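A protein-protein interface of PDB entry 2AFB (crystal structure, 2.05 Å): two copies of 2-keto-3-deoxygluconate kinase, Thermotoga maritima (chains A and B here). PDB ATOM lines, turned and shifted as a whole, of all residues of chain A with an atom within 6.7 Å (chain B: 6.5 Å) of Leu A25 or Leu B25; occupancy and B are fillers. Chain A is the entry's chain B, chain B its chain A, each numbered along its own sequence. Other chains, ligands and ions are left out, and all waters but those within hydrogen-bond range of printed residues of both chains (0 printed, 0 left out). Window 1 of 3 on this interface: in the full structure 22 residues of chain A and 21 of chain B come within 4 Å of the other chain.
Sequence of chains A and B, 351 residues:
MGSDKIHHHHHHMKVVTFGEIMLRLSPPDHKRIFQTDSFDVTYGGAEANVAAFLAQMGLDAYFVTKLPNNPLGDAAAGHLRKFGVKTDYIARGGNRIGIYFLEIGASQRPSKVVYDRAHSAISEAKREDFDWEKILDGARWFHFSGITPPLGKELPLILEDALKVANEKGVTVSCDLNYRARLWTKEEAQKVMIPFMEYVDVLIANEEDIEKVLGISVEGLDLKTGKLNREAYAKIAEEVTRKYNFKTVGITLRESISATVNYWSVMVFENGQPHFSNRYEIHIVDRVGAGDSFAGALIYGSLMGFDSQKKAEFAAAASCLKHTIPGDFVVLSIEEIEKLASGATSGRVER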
ATOM      1  N   LEU A  23      -8.528  14.425 -22.491  1.00  0.00           N
ATOM      2  CA  LEU A  23      -8.327  13.735 -23.745  1.00  0.00           C
ATOM      3  C   LEU A  23      -9.415  12.663 -23.876  1.00  0.00           C
ATOM      4  O   LEU A  23      -9.597  11.845 -22.979  1.00  0.00           O
ATOM      5  CB  LEU A  23      -6.956  13.060 -23.751  1.00  0.00           C
ATOM      6  CG  LEU A  23      -6.675  12.036 -24.836  1.00  0.00           C
ATOM      7  CD1 LEU A  23      -6.639  12.680 -26.225  1.00  0.00           C
ATOM      8  CD2 LEU A  23      -5.342  11.328 -24.507  1.00  0.00           C
ATOM      9  N   ARG A  24     -10.168  12.694 -24.959  1.00  0.00           N
ATOM     10  CA  ARG A  24     -11.145  11.646 -25.211  1.00  0.00           C
ATOM     11  C   ARG A  24     -10.669  10.742 -26.344  1.00  0.00           C
ATOM     12  O   ARG A  24     -10.267  11.236 -27.434  1.00  0.00           O
ATOM     13  CB  ARG A  24     -12.481  12.248 -25.599  1.00  0.00           C
ATOM     14  CG  ARG A  24     -13.572  11.243 -25.774  1.00  0.00           C
ATOM     15  CD  ARG A  24     -14.840  11.884 -26.364  1.00  0.00           C
ATOM     16  NE  ARG A  24     -15.075  11.390 -27.689  1.00  0.00           N
ATOM     17  CZ  ARG A  24     -16.131  11.655 -28.454  1.00  0.00           C
ATOM     18  NH1 ARG A  24     -17.103  12.444 -28.070  1.00  0.00           N
ATOM     19  NH2 ARG A  24     -16.190  11.080 -29.637  1.00  0.00           N
ATOM     20  N   LEU A  25     -10.760   9.425 -26.102  1.00  0.00           N
ATOM     21  CA  LEU A  25     -10.337   8.450 -27.043  1.00  0.00           C
ATOM     22  C   LEU A  25     -11.517   7.556 -27.393  1.00  0.00           C
ATOM     23  O   LEU A  25     -12.089   6.916 -26.542  1.00  0.00           O
ATOM     24  CB  LEU A  25      -9.212   7.617 -26.445  1.00  0.00           C
ATOM     25  CG  LEU A  25      -7.894   8.350 -26.186  1.00  0.00           C
ATOM     26  CD1 LEU A  25      -6.906   7.555 -25.316  1.00  0.00           C
ATOM     27  CD2 LEU A  25      -7.214   8.821 -27.485  1.00  0.00           C
ATOM     28  N   SER A  26     -11.901   7.513 -28.658  1.00  0.00           N
ATOM     29  CA  SER A  26     -13.018   6.698 -29.043  1.00  0.00           C
ATOM     30  C   SER A  26     -12.662   5.863 -30.270  1.00  0.00           C
ATOM     31  O   SER A  26     -12.046   6.391 -31.214  1.00  0.00           O
ATOM     32  CB  SER A  26     -14.263   7.543 -29.275  1.00  0.00           C
ATOM     33  OG  SER A  26     -14.010   8.569 -30.193  1.00  0.00           O
ATOM     34  N   PRO A  27     -13.057   4.558 -30.266  1.00  0.00           N
ATOM     35  CA  PRO A  27     -12.858   3.813 -31.494  1.00  0.00           C
ATOM     36  C   PRO A  27     -13.786   4.368 -32.569  1.00  0.00           C
ATOM     37  O   PRO A  27     -14.909   4.858 -32.254  1.00  0.00           O
ATOM     38  CB  PRO A  27     -13.307   2.390 -31.144  1.00  0.00           C
ATOM     39  CG  PRO A  27     -13.351   2.318 -29.712  1.00  0.00           C
ATOM     40  CD  PRO A  27     -13.709   3.710 -29.258  1.00  0.00           C
ATOM     41  N   ILE A  33     -13.721  -0.971 -27.772  1.00  0.00           N
ATOM     42  CA  ILE A  33     -12.318  -0.837 -27.343  1.00  0.00           C
ATOM     43  C   ILE A  33     -11.493  -2.100 -27.589  1.00  0.00           C
ATOM     44  O   ILE A  33     -10.368  -2.027 -28.095  1.00  0.00           O
ATOM     45  CB  ILE A  33     -12.301  -0.474 -25.848  1.00  0.00           C
ATOM     46  CG1 ILE A  33     -12.796   0.974 -25.680  1.00  0.00           C
ATOM     47  CG2 ILE A  33     -10.929  -0.661 -25.224  1.00  0.00           C
ATOM     48  CD1 ILE A  33     -13.302   1.363 -24.235  1.00  0.00           C
ATOM     49  N   PHE A  39      -7.760   4.892 -32.043  1.00  0.00           N
ATOM     50  CA  PHE A  39      -8.707   5.750 -31.336  1.00  0.00           C
ATOM     51  C   PHE A  39      -8.697   7.104 -32.031  1.00  0.00           C
ATOM     52  O   PHE A  39      -7.621   7.653 -32.324  1.00  0.00           O
ATOM     53  CB  PHE A  39      -8.295   5.988 -29.897  1.00  0.00           C
ATOM     54  CG  PHE A  39      -8.463   4.834 -29.018  1.00  0.00           C
ATOM     55  CD1 PHE A  39      -9.741   4.278 -28.801  1.00  0.00           C
ATOM     56  CD2 PHE A  39      -7.373   4.313 -28.340  1.00  0.00           C
ATOM     57  CE1 PHE A  39      -9.892   3.172 -27.957  1.00  0.00           C
ATOM     58  CE2 PHE A  39      -7.511   3.217 -27.466  1.00  0.00           C
ATOM     59  CZ  PHE A  39      -8.769   2.644 -27.288  1.00  0.00           C
ATOM     60  N   ASP A  40      -9.896   7.596 -32.333  1.00  0.00           N
ATOM     61  CA  ASP A  40     -10.109   9.001 -32.666  1.00  0.00           C
ATOM     62  C   ASP A  40      -9.832   9.864 -31.442  1.00  0.00           C
ATOM     63  O   ASP A  40     -10.154   9.475 -30.333  1.00  0.00           O
ATOM     64  CB  ASP A  40     -11.556   9.220 -33.132  1.00  0.00           C
ATOM     65  CG  ASP A  40     -11.873   8.432 -34.371  1.00  0.00           C
ATOM     66  OD1 ASP A  40     -10.910   8.197 -35.172  1.00  0.00           O
ATOM     67  OD2 ASP A  40     -13.068   8.063 -34.564  1.00  0.00           O
ATOM     68  N   VAL A  41      -9.224  11.028 -31.654  1.00  0.00           N
ATOM     69  CA  VAL A  41      -8.761  11.859 -30.560  1.00  0.00           C
ATOM     70  C   VAL A  41      -9.589  13.111 -30.589  1.00  0.00           C
ATOM     71  O   VAL A  41      -9.754  13.717 -31.650  1.00  0.00           O
ATOM     72  CB  VAL A  41      -7.296  12.292 -30.798  1.00  0.00           C
ATOM     73  CG1 VAL A  41      -6.885  13.411 -29.868  1.00  0.00           C
ATOM     74  CG2 VAL A  41      -6.377  11.096 -30.684  1.00  0.00           C
ATOM     75  N   THR A  42     -10.063  13.518 -29.424  1.00  0.00           N
ATOM     76  CA  THR A  42     -10.545  14.879 -29.224  1.00  0.00           C
ATOM     77  C   THR A  42     -10.337  15.236 -27.756  1.00  0.00           C
ATOM     78  O   THR A  42      -9.778  14.441 -26.970  1.00  0.00           O
ATOM     79  CB  THR A  42     -12.032  15.135 -29.732  1.00  0.00           C
ATOM     80  OG1 THR A  42     -12.304  16.545 -29.733  1.00  0.00           O
ATOM     81  CG2 THR A  42     -13.046  14.442 -28.882  1.00  0.00           C
ATOM     82  N   ILE A  99      -8.114  11.335 -18.924  1.00  0.00           N
ATOM     83  CA  ILE A  99      -8.510  10.642 -20.121  1.00  0.00           C
ATOM     84  C   ILE A  99      -9.850   9.971 -19.879  1.00  0.00           C
ATOM     85  O   ILE A  99     -10.121   9.448 -18.790  1.00  0.00           O
ATOM     86  CB  ILE A  99      -7.471   9.506 -20.499  1.00  0.00           C
ATOM     87  CG1 ILE A  99      -6.072  10.100 -20.689  1.00  0.00           C
ATOM     88  CG2 ILE A  99      -7.901   8.737 -21.782  1.00  0.00           C
ATOM     89  CD1 ILE A  99      -4.995   9.098 -21.039  1.00  0.00           C
ATOM     90  N   TYR A 100     -10.706   9.972 -20.886  1.00  0.00           N
ATOM     91  CA  TYR A 100     -11.754   8.971 -20.931  1.00  0.00           C
ATOM     92  C   TYR A 100     -11.854   8.320 -22.284  1.00  0.00           C
ATOM     93  O   TYR A 100     -11.599   8.956 -23.302  1.00  0.00           O
ATOM     94  CB  TYR A 100     -13.122   9.495 -20.491  1.00  0.00           C
ATOM     95  CG  TYR A 100     -13.889  10.413 -21.426  1.00  0.00           C
ATOM     96  CD1 TYR A 100     -13.466  11.729 -21.643  1.00  0.00           C
ATOM     97  CD2 TYR A 100     -15.097  10.026 -21.965  1.00  0.00           C
ATOM     98  CE1 TYR A 100     -14.181  12.596 -22.433  1.00  0.00           C
ATOM     99  CE2 TYR A 100     -15.851  10.914 -22.753  1.00  0.00           C
ATOM    100  CZ  TYR A 100     -15.383  12.209 -22.979  1.00  0.00           C
ATOM    101  OH  TYR A 100     -16.087  13.109 -23.790  1.00  0.00           O
ATOM    102  N   PHE A 101     -12.196   7.034 -22.251  1.00  0.00           N
ATOM    103  CA  PHE A 101     -12.381   6.226 -23.461  1.00  0.00           C
ATOM    104  C   PHE A 101     -13.881   6.087 -23.642  1.00  0.00           C
ATOM    105  O   PHE A 101     -14.587   5.820 -22.695  1.00  0.00           O
ATOM    106  CB  PHE A 101     -11.773   4.836 -23.298  1.00  0.00           C
ATOM    107  CG  PHE A 101     -10.297   4.844 -22.987  1.00  0.00           C
ATOM    108  CD1 PHE A 101      -9.845   5.008 -21.688  1.00  0.00           C
ATOM    109  CD2 PHE A 101      -9.372   4.658 -23.987  1.00  0.00           C
ATOM    110  CE1 PHE A 101      -8.497   5.024 -21.379  1.00  0.00           C
ATOM    111  CE2 PHE A 101      -8.022   4.678 -23.716  1.00  0.00           C
ATOM    112  CZ  PHE A 101      -7.570   4.872 -22.410  1.00  0.00           C
ATOM    113  N   LEU A 102     -14.343   6.225 -24.864  1.00  0.00           N
ATOM    114  CA  LEU A 102     -15.776   6.236 -25.157  1.00  0.00           C
ATOM    115  C   LEU A 102     -16.045   5.302 -26.357  1.00  0.00           C
ATOM    116  O   LEU A 102     -15.491   5.494 -27.418  1.00  0.00           O
ATOM    117  CB  LEU A 102     -16.192   7.652 -25.496  1.00  0.00           C
ATOM    118  CG  LEU A 102     -17.586   7.814 -26.075  1.00  0.00           C
ATOM    119  CD1 LEU A 102     -18.622   7.511 -24.989  1.00  0.00           C
ATOM    120  CD2 LEU A 102     -17.786   9.203 -26.651  1.00  0.00           C
ATOM    121  N   GLU A 103     -16.815   4.260 -26.134  1.00  0.00           N
ATOM    122  CA  GLU A 103     -17.403   3.442 -27.170  1.00  0.00           C
ATOM    123  C   GLU A 103     -18.722   4.106 -27.454  1.00  0.00           C
ATOM    124  O   GLU A 103     -19.545   4.259 -26.554  1.00  0.00           O
ATOM    125  CB  GLU A 103     -17.686   2.032 -26.671  1.00  0.00           C
ATOM    126  CG  GLU A 103     -16.485   1.225 -26.305  1.00  0.00           C
ATOM    127  CD  GLU A 103     -16.804  -0.199 -25.782  1.00  0.00           C
ATOM    128  OE1 GLU A 103     -17.962  -0.476 -25.326  1.00  0.00           O
ATOM    129  OE2 GLU A 103     -15.855  -1.045 -25.799  1.00  0.00           O
ATOM    130  N   LEU B  23      -0.800   0.034 -22.691  1.00  0.00           N
ATOM    131  CA  LEU B  23      -1.394   0.566 -23.918  1.00  0.00           C
ATOM    132  C   LEU B  23      -0.446   1.558 -24.588  1.00  0.00           C
ATOM    133  O   LEU B  23      -0.030   2.515 -23.937  1.00  0.00           O
ATOM    134  CB  LEU B  23      -2.681   1.296 -23.585  1.00  0.00           C
ATOM    135  CG  LEU B  23      -3.306   2.110 -24.761  1.00  0.00           C
ATOM    136  CD1 LEU B  23      -3.820   1.276 -25.897  1.00  0.00           C
ATOM    137  CD2 LEU B  23      -4.438   2.976 -24.219  1.00  0.00           C
ATOM    138  N   ARG B  24      -0.137   1.364 -25.877  1.00  0.00           N
ATOM    139  CA  ARG B  24       0.701   2.294 -26.604  1.00  0.00           C
ATOM    140  C   ARG B  24      -0.117   3.094 -27.635  1.00  0.00           C
ATOM    141  O   ARG B  24      -0.837   2.538 -28.450  1.00  0.00           O
ATOM    142  CB  ARG B  24       1.816   1.592 -27.301  1.00  0.00           C
ATOM    143  CG  ARG B  24       2.941   2.540 -27.682  1.00  0.00           C
ATOM    144  CD  ARG B  24       3.956   1.846 -28.574  1.00  0.00           C
ATOM    145  NE  ARG B  24       3.652   2.050 -29.961  1.00  0.00           N
ATOM    146  CZ  ARG B  24       4.404   1.693 -30.996  1.00  0.00           C
ATOM    147  NH1 ARG B  24       5.558   1.046 -30.859  1.00  0.00           N
ATOM    148  NH2 ARG B  24       3.971   2.003 -32.211  1.00  0.00           N
ATOM    149  N   LEU B  25       0.043   4.409 -27.574  1.00  0.00           N
ATOM    150  CA  LEU B  25      -0.734   5.326 -28.392  1.00  0.00           C
ATOM    151  C   LEU B  25       0.252   6.113 -29.216  1.00  0.00           C
ATOM    152  O   LEU B  25       1.059   6.840 -28.660  1.00  0.00           O
ATOM    153  CB  LEU B  25      -1.575   6.210 -27.539  1.00  0.00           C
ATOM    154  CG  LEU B  25      -2.708   5.586 -26.679  1.00  0.00           C
ATOM    155  CD1 LEU B  25      -3.333   6.692 -25.906  1.00  0.00           C
ATOM    156  CD2 LEU B  25      -3.778   4.832 -27.481  1.00  0.00           C
ATOM    157  N   SER B  26       0.246   5.921 -30.536  1.00  0.00           N
ATOM    158  CA  SER B  26       1.199   6.623 -31.402  1.00  0.00           C
ATOM    159  C   SER B  26       0.495   7.306 -32.549  1.00  0.00           C
ATOM    160  O   SER B  26      -0.391   6.695 -33.138  1.00  0.00           O
ATOM    161  CB  SER B  26       2.301   5.694 -31.932  1.00  0.00           C
ATOM    162  OG  SER B  26       1.709   4.526 -32.479  1.00  0.00           O
ATOM    163  N   PRO B  27       0.842   8.607 -32.836  1.00  0.00           N
ATOM    164  CA  PRO B  27       0.201   9.170 -33.980  1.00  0.00           C
ATOM    165  C   PRO B  27       0.705   8.472 -35.268  1.00  0.00           C
ATOM    166  O   PRO B  27       1.821   7.973 -35.285  1.00  0.00           O
ATOM    167  CB  PRO B  27       0.636  10.638 -33.943  1.00  0.00           C
ATOM    168  CG  PRO B  27       1.176  10.921 -32.535  1.00  0.00           C
ATOM    169  CD  PRO B  27       1.727   9.589 -32.150  1.00  0.00           C
ATOM    170  N   ILE B  33       2.059  14.486 -31.406  1.00  0.00           N
ATOM    171  CA  ILE B  33       0.861  14.403 -30.591  1.00  0.00           C
ATOM    172  C   ILE B  33      -0.025  15.614 -30.777  1.00  0.00           C
ATOM    173  O   ILE B  33      -1.233  15.483 -30.952  1.00  0.00           O
ATOM    174  CB  ILE B  33       1.219  14.177 -29.094  1.00  0.00           C
ATOM    175  CG1 ILE B  33       1.834  12.774 -28.942  1.00  0.00           C
ATOM    176  CG2 ILE B  33      -0.028  14.364 -28.216  1.00  0.00           C
ATOM    177  CD1 ILE B  33       2.828  12.510 -27.683  1.00  0.00           C
ATOM    178  N   PHE B  39      -4.744   8.174 -32.792  1.00  0.00           N
ATOM    179  CA  PHE B  39      -3.645   7.367 -32.302  1.00  0.00           C
ATOM    180  C   PHE B  39      -3.860   5.929 -32.776  1.00  0.00           C
ATOM    181  O   PHE B  39      -4.957   5.379 -32.603  1.00  0.00           O
ATOM    182  CB  PHE B  39      -3.600   7.302 -30.777  1.00  0.00           C
ATOM    183  CG  PHE B  39      -3.197   8.581 -30.122  1.00  0.00           C
ATOM    184  CD1 PHE B  39      -1.992   9.182 -30.441  1.00  0.00           C
ATOM    185  CD2 PHE B  39      -4.036   9.185 -29.155  1.00  0.00           C
ATOM    186  CE1 PHE B  39      -1.607  10.398 -29.854  1.00  0.00           C
ATOM    187  CE2 PHE B  39      -3.659  10.369 -28.545  1.00  0.00           C
ATOM    188  CZ  PHE B  39      -2.430  10.996 -28.906  1.00  0.00           C
ATOM    189  N   ASP B  40      -2.801   5.364 -33.374  1.00  0.00           N
ATOM    190  CA  ASP B  40      -2.617   3.948 -33.564  1.00  0.00           C
ATOM    191  C   ASP B  40      -2.482   3.330 -32.195  1.00  0.00           C
ATOM    192  O   ASP B  40      -1.867   3.907 -31.328  1.00  0.00           O
ATOM    193  CB  ASP B  40      -1.370   3.686 -34.389  1.00  0.00           C
ATOM    194  CG  ASP B  40      -1.504   4.225 -35.815  1.00  0.00           C
ATOM    195  OD1 ASP B  40      -2.629   4.148 -36.330  1.00  0.00           O
ATOM    196  OD2 ASP B  40      -0.525   4.678 -36.433  1.00  0.00           O
ATOM    197  N   VAL B  41      -3.100   2.169 -32.043  1.00  0.00           N
ATOM    198  CA  VAL B  41      -3.226   1.441 -30.796  1.00  0.00           C
ATOM    199  C   VAL B  41      -2.476   0.132 -30.915  1.00  0.00           C
ATOM    200  O   VAL B  41      -2.578  -0.546 -31.900  1.00  0.00           O
ATOM    201  CB  VAL B  41      -4.704   1.080 -30.485  1.00  0.00           C
ATOM    202  CG1 VAL B  41      -4.808   0.040 -29.379  1.00  0.00           C
ATOM    203  CG2 VAL B  41      -5.464   2.336 -30.075  1.00  0.00           C
ATOM    204  N   THR B  42      -1.687  -0.160 -29.901  1.00  0.00           N
ATOM    205  CA  THR B  42      -1.104  -1.467 -29.686  1.00  0.00           C
ATOM    206  C   THR B  42      -0.783  -1.652 -28.215  1.00  0.00           C
ATOM    207  O   THR B  42      -1.044  -0.772 -27.385  1.00  0.00           O
ATOM    208  CB  THR B  42       0.117  -1.760 -30.611  1.00  0.00           C
ATOM    209  OG1 THR B  42       0.362  -3.181 -30.609  1.00  0.00           O
ATOM    210  CG2 THR B  42       1.387  -0.991 -30.169  1.00  0.00           C
ATOM    211  N   ILE B  99      -0.192   3.479 -19.655  1.00  0.00           N
ATOM    212  CA  ILE B  99      -0.204   3.961 -21.007  1.00  0.00           C
ATOM    213  C   ILE B  99       1.110   4.654 -21.344  1.00  0.00           C
ATOM    214  O   ILE B  99       1.692   5.333 -20.498  1.00  0.00           O
ATOM    215  CB  ILE B  99      -1.316   5.059 -21.226  1.00  0.00           C
ATOM    216  CG1 ILE B  99      -2.681   4.528 -20.821  1.00  0.00           C
ATOM    217  CG2 ILE B  99      -1.246   5.545 -22.654  1.00  0.00           C
ATOM    218  CD1 ILE B  99      -3.809   5.600 -20.895  1.00  0.00           C
ATOM    219  N   TYR B 100       1.544   4.543 -22.596  1.00  0.00           N
ATOM    220  CA  TYR B 100       2.494   5.486 -23.109  1.00  0.00           C
ATOM    221  C   TYR B 100       2.165   5.976 -24.477  1.00  0.00           C
ATOM    222  O   TYR B 100       1.616   5.232 -25.294  1.00  0.00           O
ATOM    223  CB  TYR B 100       3.923   4.973 -23.040  1.00  0.00           C
ATOM    224  CG  TYR B 100       4.408   3.915 -23.995  1.00  0.00           C
ATOM    225  CD1 TYR B 100       4.000   2.584 -23.881  1.00  0.00           C
ATOM    226  CD2 TYR B 100       5.339   4.233 -24.987  1.00  0.00           C
ATOM    227  CE1 TYR B 100       4.524   1.592 -24.719  1.00  0.00           C
ATOM    228  CE2 TYR B 100       5.886   3.248 -25.822  1.00  0.00           C
ATOM    229  CZ  TYR B 100       5.481   1.930 -25.685  1.00  0.00           C
ATOM    230  OH  TYR B 100       5.990   0.959 -26.541  1.00  0.00           O
ATOM    231  N   PHE B 101       2.475   7.259 -24.683  1.00  0.00           N
ATOM    232  CA  PHE B 101       2.282   7.905 -25.975  1.00  0.00           C
ATOM    233  C   PHE B 101       3.637   7.943 -26.633  1.00  0.00           C
ATOM    234  O   PHE B 101       4.611   8.329 -26.026  1.00  0.00           O
ATOM    235  CB  PHE B 101       1.776   9.317 -25.819  1.00  0.00           C
ATOM    236  CG  PHE B 101       0.462   9.417 -25.104  1.00  0.00           C
ATOM    237  CD1 PHE B 101       0.406   9.307 -23.752  1.00  0.00           C
ATOM    238  CD2 PHE B 101      -0.736   9.598 -25.800  1.00  0.00           C
ATOM    239  CE1 PHE B 101      -0.805   9.386 -23.070  1.00  0.00           C
ATOM    240  CE2 PHE B 101      -1.948   9.685 -25.114  1.00  0.00           C
ATOM    241  CZ  PHE B 101      -1.970   9.550 -23.744  1.00  0.00           C
ATOM    242  N   LEU B 102       3.690   7.562 -27.881  1.00  0.00           N
ATOM    243  CA  LEU B 102       4.933   7.531 -28.610  1.00  0.00           C
ATOM    244  C   LEU B 102       4.835   8.307 -29.909  1.00  0.00           C
ATOM    245  O   LEU B 102       3.946   8.036 -30.743  1.00  0.00           O
ATOM    246  CB  LEU B 102       5.299   6.079 -28.913  1.00  0.00           C
ATOM    247  CG  LEU B 102       6.453   5.935 -29.918  1.00  0.00           C
ATOM    248  CD1 LEU B 102       7.738   6.235 -29.187  1.00  0.00           C
ATOM    249  CD2 LEU B 102       6.472   4.473 -30.488  1.00  0.00           C
ATOM    250  N   GLU B 103       5.748   9.271 -30.083  1.00  0.00           N
ATOM    251  CA  GLU B 103       5.937   9.980 -31.334  1.00  0.00           C
ATOM    252  C   GLU B 103       7.098   9.330 -31.978  1.00  0.00           C
ATOM    253  O   GLU B 103       8.206   9.349 -31.441  1.00  0.00           O
ATOM    254  CB  GLU B 103       6.290  11.432 -31.146  1.00  0.00           C
ATOM    255  CG  GLU B 103       5.185  12.315 -30.624  1.00  0.00           C
ATOM    256  CD  GLU B 103       5.627  13.785 -30.437  1.00  0.00           C
ATOM    257  OE1 GLU B 103       6.861  14.046 -30.263  1.00  0.00           O
ATOM    258  OE2 GLU B 103       4.734  14.667 -30.431  1.00  0.00           O
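N of Phe A39 is in hydrogen-bond range of O of Phe B39, at 2.9 Å.
Leu A23 touches Phe B101, and with the chains exchanged Phe A101 touches Leu B23.
Leu A25 touches Phe B39, and with the chains exchanged Phe A39 touches Leu B25.
Phe A39 touches its own counterpart, Phe B39.
Phe A39 touches Val B41, and with the chains exchanged Val A41 touches Phe B39.
15 positions are printed for both chains.
Leu A25 touches just these residues of chain B: Leu B25 and Phe B39.
Pro A27 touches none of the printed residues of chain B.
Of the printed residues of chain B, Ile A99 touches Ile B99.
Leu B25 touches two residues of chain A.
Asp B40 touches none of the printed residues of chain A.
Of the printed residues of chain A, Ile B99 touches Ile A99 (3.7 Å).
The nearest printed residue of chain A that does not touch Ile B99 is Phe A101 (4.1 Å).
Leu A23 touches Phe B101.
Leu B25 touches Leu A25 (CD1 to CD1, 3.7 Å).
Leu A25 touches Phe B39 (CD2 to CD2, 3.6 Å).
Phe A39 touches Leu B25 (CD2 to CD2, 3.7 Å).
Val B41 touches Phe A39 (CG2 to CD2, 3.3 Å).
CG2 of Val A41 touches CD2 of Phe B39 (3.4 Å).
CD1 of Ile A99 touches CD1 of Ile B99, at 3.7 Å.
Phe A101 touches Leu B23.
The backbone NH (N) of Tyr B100 sits at hydrogen-bond distance from the backbone carbonyl oxygen (O) of Leu B23.
N of Leu B25 is in hydrogen-bond range of O of Tyr B100 (2.9 Å).
The backbone carbonyl oxygen (O) of Leu B25 lies within hydrogen-bond range of the backbone NH (N) of Leu B102, at 2.8 Å.
N of Tyr A100 is in hydrogen-bond range of O of Leu A23, at 3.0 Å.
N of Leu A25 sits at hydrogen-bond distance from O of Tyr A100 (3.0 Å).
The backbone carbonyl oxygen (O) of Leu A25 lies within hydrogen-bond range of the backbone NH (N) of Leu A102.
Of the 15 printed residues of chain B, 6 touch a printed residue of chain A.
Among the printed residues, no Asp or Glu carboxylate lies within 4 Å of a Lys or Arg side-chain nitrogen of the other chain.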
